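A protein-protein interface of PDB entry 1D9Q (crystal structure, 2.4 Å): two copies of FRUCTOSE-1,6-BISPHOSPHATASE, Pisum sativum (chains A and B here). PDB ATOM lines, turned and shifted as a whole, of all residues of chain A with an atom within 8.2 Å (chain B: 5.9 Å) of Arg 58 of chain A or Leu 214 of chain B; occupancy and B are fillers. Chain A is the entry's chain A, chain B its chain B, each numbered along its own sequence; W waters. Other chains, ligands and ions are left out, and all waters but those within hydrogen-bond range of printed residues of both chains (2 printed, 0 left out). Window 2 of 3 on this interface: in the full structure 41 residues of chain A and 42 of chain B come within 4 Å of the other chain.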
ATOM      1  N   GLN A  51      18.868   2.379 -18.280  1.00  0.00           N
ATOM      2  CA  GLN A  51      19.089   0.958 -18.520  1.00  0.00           C
ATOM      3  C   GLN A  51      18.315   0.404 -19.718  1.00  0.00           C
ATOM      4  O   GLN A  51      18.837  -0.417 -20.470  1.00  0.00           O
ATOM      5  CB  GLN A  51      18.731   0.153 -17.277  1.00  0.00           C
ATOM      6  CG  GLN A  51      19.568   0.486 -16.063  1.00  0.00           C
ATOM      7  CD  GLN A  51      19.468  -0.565 -14.964  1.00  0.00           C
ATOM      8  OE1 GLN A  51      19.267  -1.757 -15.226  1.00  0.00           O
ATOM      9  NE2 GLN A  51      19.634  -0.127 -13.725  1.00  0.00           N
ATOM     10  N   ILE A  52      17.055   0.810 -19.853  1.00  0.00           N
ATOM     11  CA  ILE A  52      16.221   0.370 -20.961  1.00  0.00           C
ATOM     12  C   ILE A  52      16.792   0.926 -22.267  1.00  0.00           C
ATOM     13  O   ILE A  52      16.785   0.243 -23.283  1.00  0.00           O
ATOM     14  CB  ILE A  52      14.757   0.809 -20.773  1.00  0.00           C
ATOM     15  CG1 ILE A  52      14.173   0.106 -19.550  1.00  0.00           C
ATOM     16  CG2 ILE A  52      13.930   0.484 -22.009  1.00  0.00           C
ATOM     17  CD1 ILE A  52      12.805   0.585 -19.156  1.00  0.00           C
ATOM     18  N   ALA A  53      17.322   2.146 -22.225  1.00  0.00           N
ATOM     19  CA  ALA A  53      17.924   2.752 -23.414  1.00  0.00           C
ATOM     20  C   ALA A  53      19.055   1.867 -23.953  1.00  0.00           C
ATOM     21  O   ALA A  53      19.151   1.630 -25.162  1.00  0.00           O
ATOM     22  CB  ALA A  53      18.458   4.138 -23.081  1.00  0.00           C
ATOM     23  N   SER A  54      19.885   1.368 -23.036  1.00  0.00           N
ATOM     24  CA  SER A  54      21.019   0.499 -23.354  1.00  0.00           C
ATOM     25  C   SER A  54      20.545  -0.825 -23.946  1.00  0.00           C
ATOM     26  O   SER A  54      21.166  -1.346 -24.876  1.00  0.00           O
ATOM     27  CB  SER A  54      21.870   0.245 -22.097  1.00  0.00           C
ATOM     28  OG  SER A  54      23.051  -0.478 -22.400  1.00  0.00           O
ATOM     29  N   LEU A  55      19.449  -1.359 -23.402  1.00  0.00           N
ATOM     30  CA  LEU A  55      18.863  -2.608 -23.884  1.00  0.00           C
ATOM     31  C   LEU A  55      18.422  -2.458 -25.336  1.00  0.00           C
ATOM     32  O   LEU A  55      18.639  -3.348 -26.157  1.00  0.00           O
ATOM     33  CB  LEU A  55      17.652  -3.005 -23.035  1.00  0.00           C
ATOM     34  CG  LEU A  55      17.900  -3.435 -21.592  1.00  0.00           C
ATOM     35  CD1 LEU A  55      16.568  -3.713 -20.908  1.00  0.00           C
ATOM     36  CD2 LEU A  55      18.782  -4.661 -21.570  1.00  0.00           C
ATOM     37  N   VAL A  56      17.776  -1.333 -25.629  1.00  0.00           N
ATOM     38  CA  VAL A  56      17.297  -1.020 -26.970  1.00  0.00           C
ATOM     39  C   VAL A  56      18.459  -0.862 -27.958  1.00  0.00           C
ATOM     40  O   VAL A  56      18.408  -1.383 -29.071  1.00  0.00           O
ATOM     41  CB  VAL A  56      16.430   0.266 -26.952  1.00  0.00           C
ATOM     42  CG1 VAL A  56      16.144   0.734 -28.368  1.00  0.00           C
ATOM     43  CG2 VAL A  56      15.117   0.004 -26.212  1.00  0.00           C
ATOM     44  N   GLN A  57      19.508  -0.171 -27.524  1.00  0.00           N
ATOM     45  CA  GLN A  57      20.690   0.052 -28.344  1.00  0.00           C
ATOM     46  C   GLN A  57      21.454  -1.223 -28.709  1.00  0.00           C
ATOM     47  O   GLN A  57      22.040  -1.315 -29.790  1.00  0.00           O
ATOM     48  CB  GLN A  57      21.634   1.008 -27.635  1.00  0.00           C
ATOM     49  CG  GLN A  57      21.061   2.383 -27.446  1.00  0.00           C
ATOM     50  CD  GLN A  57      21.928   3.271 -26.577  1.00  0.00           C
ATOM     51  OE1 GLN A  57      22.924   2.830 -26.000  1.00  0.00           O
ATOM     52  NE2 GLN A  57      21.541   4.533 -26.467  1.00  0.00           N
ATOM     53  N   ARG A  58      21.432  -2.210 -27.821  1.00  0.00           N
ATOM     54  CA  ARG A  58      22.146  -3.464 -28.057  1.00  0.00           C
ATOM     55  C   ARG A  58      21.264  -4.648 -28.427  1.00  0.00           C
ATOM     56  O   ARG A  58      21.749  -5.771 -28.486  1.00  0.00           O
ATOM     57  CB  ARG A  58      22.959  -3.847 -26.822  1.00  0.00           C
ATOM     58  CG  ARG A  58      23.916  -2.786 -26.320  1.00  0.00           C
ATOM     59  CD  ARG A  58      24.736  -3.323 -25.158  1.00  0.00           C
ATOM     60  NE  ARG A  58      25.733  -4.312 -25.578  1.00  0.00           N
ATOM     61  CZ  ARG A  58      25.717  -5.604 -25.253  1.00  0.00           C
ATOM     62  NH1 ARG A  58      24.748  -6.106 -24.493  1.00  0.00           N
ATOM     63  NH2 ARG A  58      26.688  -6.397 -25.676  1.00  0.00           N
ATOM     64  N   ALA A  59      19.980  -4.407 -28.676  1.00  0.00           N
ATOM     65  CA  ALA A  59      19.050  -5.481 -29.016  1.00  0.00           C
ATOM     66  C   ALA A  59      19.551  -6.491 -30.060  1.00  0.00           C
ATOM     67  O   ALA A  59      19.476  -7.692 -29.836  1.00  0.00           O
ATOM     68  CB  ALA A  59      17.722  -4.895 -29.439  1.00  0.00           C
ATOM     69  N   ASN A  60      20.080  -6.009 -31.181  1.00  0.00           N
ATOM     70  CA  ASN A  60      20.577  -6.885 -32.245  1.00  0.00           C
ATOM     71  C   ASN A  60      21.693  -7.819 -31.785  1.00  0.00           C
ATOM     72  O   ASN A  60      21.760  -8.981 -32.188  1.00  0.00           O
ATOM     73  CB  ASN A  60      21.086  -6.056 -33.430  1.00  0.00           C
ATOM     74  CG  ASN A  60      19.979  -5.322 -34.156  1.00  0.00           C
ATOM     75  OD1 ASN A  60      18.799  -5.635 -33.988  1.00  0.00           O
ATOM     76  ND2 ASN A  60      20.356  -4.349 -34.986  1.00  0.00           N
ATOM     77  N   ILE A  61      22.599  -7.273 -30.986  1.00  0.00           N
ATOM     78  CA  ILE A  61      23.739  -8.007 -30.454  1.00  0.00           C
ATOM     79  C   ILE A  61      23.278  -9.021 -29.407  1.00  0.00           C
ATOM     80  O   ILE A  61      23.643 -10.191 -29.468  1.00  0.00           O
ATOM     81  CB  ILE A  61      24.757  -7.024 -29.825  1.00  0.00           C
ATOM     82  CG1 ILE A  61      25.197  -6.000 -30.864  1.00  0.00           C
ATOM     83  CG2 ILE A  61      25.972  -7.759 -29.295  1.00  0.00           C
ATOM     84  CD1 ILE A  61      26.019  -4.880 -30.297  1.00  0.00           C
ATOM     85  N   SER A  62      22.458  -8.573 -28.461  1.00  0.00           N
ATOM     86  CA  SER A  62      21.947  -9.445 -27.413  1.00  0.00           C
ATOM     87  C   SER A  62      21.154 -10.605 -27.993  1.00  0.00           C
ATOM     88  O   SER A  62      21.101 -11.676 -27.393  1.00  0.00           O
ATOM     89  CB  SER A  62      21.074  -8.663 -26.432  1.00  0.00           C
ATOM     90  OG  SER A  62      21.848  -7.732 -25.701  1.00  0.00           O
ATOM     91  N   ASN A  63      20.557 -10.395 -29.166  1.00  0.00           N
ATOM     92  CA  ASN A  63      19.767 -11.434 -29.823  1.00  0.00           C
ATOM     93  C   ASN A  63      20.610 -12.459 -30.574  1.00  0.00           C
ATOM     94  O   ASN A  63      20.100 -13.503 -30.989  1.00  0.00           O
ATOM     95  CB  ASN A  63      18.702 -10.818 -30.733  1.00  0.00           C
ATOM     96  CG  ASN A  63      17.645 -10.050 -29.949  1.00  0.00           C
ATOM     97  OD1 ASN A  63      17.318 -10.398 -28.809  1.00  0.00           O
ATOM     98  ND2 ASN A  63      17.118  -8.987 -30.552  1.00  0.00           N
ATOM     99  N   LEU A  64      21.897 -12.158 -30.750  1.00  0.00           N
ATOM    100  CA  LEU A  64      22.818 -13.075 -31.417  1.00  0.00           C
ATOM    101  C   LEU A  64      23.066 -14.250 -30.485  1.00  0.00           C
ATOM    102  O   LEU A  64      23.229 -15.388 -30.925  1.00  0.00           O
ATOM    103  CB  LEU A  64      24.155 -12.403 -31.702  1.00  0.00           C
ATOM    104  CG  LEU A  64      24.252 -11.435 -32.871  1.00  0.00           C
ATOM    105  CD1 LEU A  64      25.695 -10.948 -32.959  1.00  0.00           C
ATOM    106  CD2 LEU A  64      23.825 -12.123 -34.161  1.00  0.00           C
ATOM    107  N   LEU A  81      11.489  -7.755 -24.988  1.00  0.00           N
ATOM    108  CA  LEU A  81      12.179  -6.553 -24.532  1.00  0.00           C
ATOM    109  C   LEU A  81      11.208  -5.850 -23.572  1.00  0.00           C
ATOM    110  O   LEU A  81      11.627  -5.167 -22.633  1.00  0.00           O
ATOM    111  CB  LEU A  81      12.520  -5.653 -25.720  1.00  0.00           C
ATOM    112  CG  LEU A  81      13.694  -4.688 -25.565  1.00  0.00           C
ATOM    113  CD1 LEU A  81      14.893  -5.407 -24.958  1.00  0.00           C
ATOM    114  CD2 LEU A  81      14.055  -4.123 -26.934  1.00  0.00           C
ATOM    115  N   SER B 195      19.252   2.824 -32.506  1.00  0.00           N
ATOM    116  CA  SER B 195      20.351   1.895 -32.676  1.00  0.00           C
ATOM    117  C   SER B 195      21.261   2.512 -33.757  1.00  0.00           C
ATOM    118  O   SER B 195      20.789   3.292 -34.591  1.00  0.00           O
ATOM    119  CB  SER B 195      19.774   0.565 -33.172  1.00  0.00           C
ATOM    120  OG  SER B 195      20.634  -0.509 -32.880  1.00  0.00           O
ATOM    121  N   THR B 210      25.968  -3.863 -36.121  1.00  0.00           N
ATOM    122  CA  THR B 210      25.379  -3.074 -35.048  1.00  0.00           C
ATOM    123  C   THR B 210      26.473  -2.592 -34.100  1.00  0.00           C
ATOM    124  O   THR B 210      27.339  -3.366 -33.702  1.00  0.00           O
ATOM    125  CB  THR B 210      24.363  -3.902 -34.233  1.00  0.00           C
ATOM    126  OG1 THR B 210      23.320  -4.363 -35.096  1.00  0.00           O
ATOM    127  CG2 THR B 210      23.753  -3.067 -33.125  1.00  0.00           C
ATOM    128  N   LEU B 211      26.436  -1.309 -33.752  1.00  0.00           N
ATOM    129  CA  LEU B 211      27.416  -0.738 -32.832  1.00  0.00           C
ATOM    130  C   LEU B 211      27.112  -1.107 -31.384  1.00  0.00           C
ATOM    131  O   LEU B 211      25.989  -0.935 -30.913  1.00  0.00           O
ATOM    132  CB  LEU B 211      27.449   0.784 -32.958  1.00  0.00           C
ATOM    133  CG  LEU B 211      28.438   1.530 -32.057  1.00  0.00           C
ATOM    134  CD1 LEU B 211      29.874   1.208 -32.467  1.00  0.00           C
ATOM    135  CD2 LEU B 211      28.186   3.029 -32.147  1.00  0.00           C
ATOM    136  N   ASP B 212      28.117  -1.633 -30.694  1.00  0.00           N
ATOM    137  CA  ASP B 212      27.973  -1.999 -29.297  1.00  0.00           C
ATOM    138  C   ASP B 212      28.395  -0.767 -28.525  1.00  0.00           C
ATOM    139  O   ASP B 212      29.576  -0.442 -28.472  1.00  0.00           O
ATOM    140  CB  ASP B 212      28.883  -3.169 -28.951  1.00  0.00           C
ATOM    141  CG  ASP B 212      28.439  -3.884 -27.704  1.00  0.00           C
ATOM    142  OD1 ASP B 212      28.022  -3.202 -26.752  1.00  0.00           O
ATOM    143  OD2 ASP B 212      28.484  -5.129 -27.682  1.00  0.00           O
ATOM    144  N   PRO B 213      27.434  -0.070 -27.902  1.00  0.00           N
ATOM    145  CA  PRO B 213      27.673   1.153 -27.123  1.00  0.00           C
ATOM    146  C   PRO B 213      28.756   0.945 -26.061  1.00  0.00           C
ATOM    147  O   PRO B 213      29.595   1.824 -25.802  1.00  0.00           O
ATOM    148  CB  PRO B 213      26.305   1.394 -26.479  1.00  0.00           C
ATOM    149  CG  PRO B 213      25.346   0.755 -27.453  1.00  0.00           C
ATOM    150  CD  PRO B 213      26.056  -0.537 -27.700  1.00  0.00           C
ATOM    151  N   LEU B 214      28.738  -0.266 -25.508  1.00  0.00           N
ATOM    152  CA  LEU B 214      29.640  -0.724 -24.463  1.00  0.00           C
ATOM    153  C   LEU B 214      31.123  -0.731 -24.794  1.00  0.00           C
ATOM    154  O   LEU B 214      31.915  -0.079 -24.124  1.00  0.00           O
ATOM    155  CB  LEU B 214      29.243  -2.142 -24.036  1.00  0.00           C
ATOM    156  CG  LEU B 214      27.883  -2.315 -23.352  1.00  0.00           C
ATOM    157  CD1 LEU B 214      27.697  -3.777 -22.955  1.00  0.00           C
ATOM    158  CD2 LEU B 214      27.806  -1.422 -22.119  1.00  0.00           C
ATOM    159  N   TYR B 215      31.473  -1.465 -25.847  1.00  0.00           N
ATOM    160  CA  TYR B 215      32.850  -1.659 -26.272  1.00  0.00           C
ATOM    161  C   TYR B 215      33.309  -0.846 -27.479  1.00  0.00           C
ATOM    162  O   TYR B 215      34.441  -0.988 -27.942  1.00  0.00           O
ATOM    163  CB  TYR B 215      33.046  -3.157 -26.485  1.00  0.00           C
ATOM    164  CG  TYR B 215      32.458  -3.949 -25.332  1.00  0.00           C
ATOM    165  CD1 TYR B 215      31.397  -4.840 -25.529  1.00  0.00           C
ATOM    166  CD2 TYR B 215      32.942  -3.777 -24.030  1.00  0.00           C
ATOM    167  CE1 TYR B 215      30.836  -5.542 -24.458  1.00  0.00           C
ATOM    168  CE2 TYR B 215      32.391  -4.471 -22.951  1.00  0.00           C
ATOM    169  CZ  TYR B 215      31.340  -5.353 -23.173  1.00  0.00           C
ATOM    170  OH  TYR B 215      30.816  -6.066 -22.115  1.00  0.00           O
ATOM    171  N   GLY B 216      32.433   0.026 -27.963  1.00  0.00           N
ATOM    172  CA  GLY B 216      32.761   0.874 -29.096  1.00  0.00           C
ATOM    173  C   GLY B 216      33.195   0.180 -30.375  1.00  0.00           C
ATOM    174  O   GLY B 216      34.087   0.672 -31.068  1.00  0.00           O
HETATM  175  O   HOH W   1      19.959  -3.064 -31.791  1.00  0.00           O
HETATM  176  O   HOH W   2      23.668   0.415 -31.277  1.00  0.00           O
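The side-chain hydroxyl (OG1) of Thr 210 of chain B sits at hydrogen-bond distance from the side-chain amide nitrogen (ND2) of Asn 60 of chain A (3.0 Å).
The guanidinium group of Arg 58 of chain A lies within salt-bridge range of the side-chain carboxylate of Asp 212 of chain B (2.8 Å).
The backbone carbonyl oxygen (O) of Gln 57 of chain A is in hydrogen-bond range of the side-chain hydroxyl (OG) of Ser 195 of chain B.
The side-chain hydroxyl (OG) of Ser 62 of chain A lies within hydrogen-bond range of the backbone carbonyl oxygen (O) of Arg 58 of chain A (3.4 Å).
N of Leu 214 of chain B sits close to OD1 of Asp 212 of chain B.
Gln 57 of chain A touches Pro 213 of chain B (OE1 to CG, 3.5 Å).
CG of Arg 58 of chain A touches CD of Pro 213 of chain B, at 3.4 Å.
Arg 58 of chain A touches Leu 214 of chain B.
Ile 61 of chain A touches Thr 210 of chain B.
Leu 211 of chain B touches Ile 61 of chain A.
Ile 61 of chain A touches Asp 212 of chain B.
Of chain B, only Asp 212, Pro 213 and Leu 214 come within 4 Å of Arg 58 of chain A.
Leu 214 of chain B touches just one residue of chain A: Arg 58 (3.3 Å).
Of the printed residues of chain A, Pro 213 of chain B touches Gln 57 (3.5 Å) and Arg 58 (3.4 Å).
Of the printed residues of chain B, Ile 61 of chain A touches Thr 210, Leu 211 and Asp 212.
Of the printed residues of chain B, Gln 57 of chain A touches Ser 195 (3.5 Å) and Pro 213 (3.5 Å).
Printed residues of chain B within 4 Å of Asn 60 of chain A: Thr 210 (3.0 Å).
Of the printed residues of chain A, Leu 211 of chain B touches Ile 61 (3.99 Å).
Gln 51 of chain A touches none of the printed residues of chain B.
Hydrophobic or aromatic side chains of chain A within 4 Å of the printed part of chain B: Ile 61.
Of the 8 printed residues of chain B, 6 touch a printed residue of chain A.
Hydrophobic or aromatic side chains of chain B within 4 Å of the printed part of chain A: Pro 213 and Leu 214.
Among the printed residues, 9 pairs touch across the chains.
Among the printed residues, Asp or Glu carboxylates within 4 Å of a Lys or Arg side-chain nitrogen of the other chain: Arg 58 of chain A with Asp 212 of chain B (2.8 Å).
No position is printed for both chains.
Of the 9 pairs that touch across the chains among the printed residues, none has its exchanged pair printed and touching as well.
Water W2 lies within hydrogen-bond range of the backbone carbonyl oxygen (O) of Leu 211 of chain B (2.7 Å) and the backbone carbonyl oxygen (O) of Gln 57 of chain A (2.8 Å).
Water W1 lies within hydrogen-bond range of OG of Ser 195 of chain B, N of Asn 60 of chain A, O of Gln 57 of chain A and N of Ala 59 of chain A.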
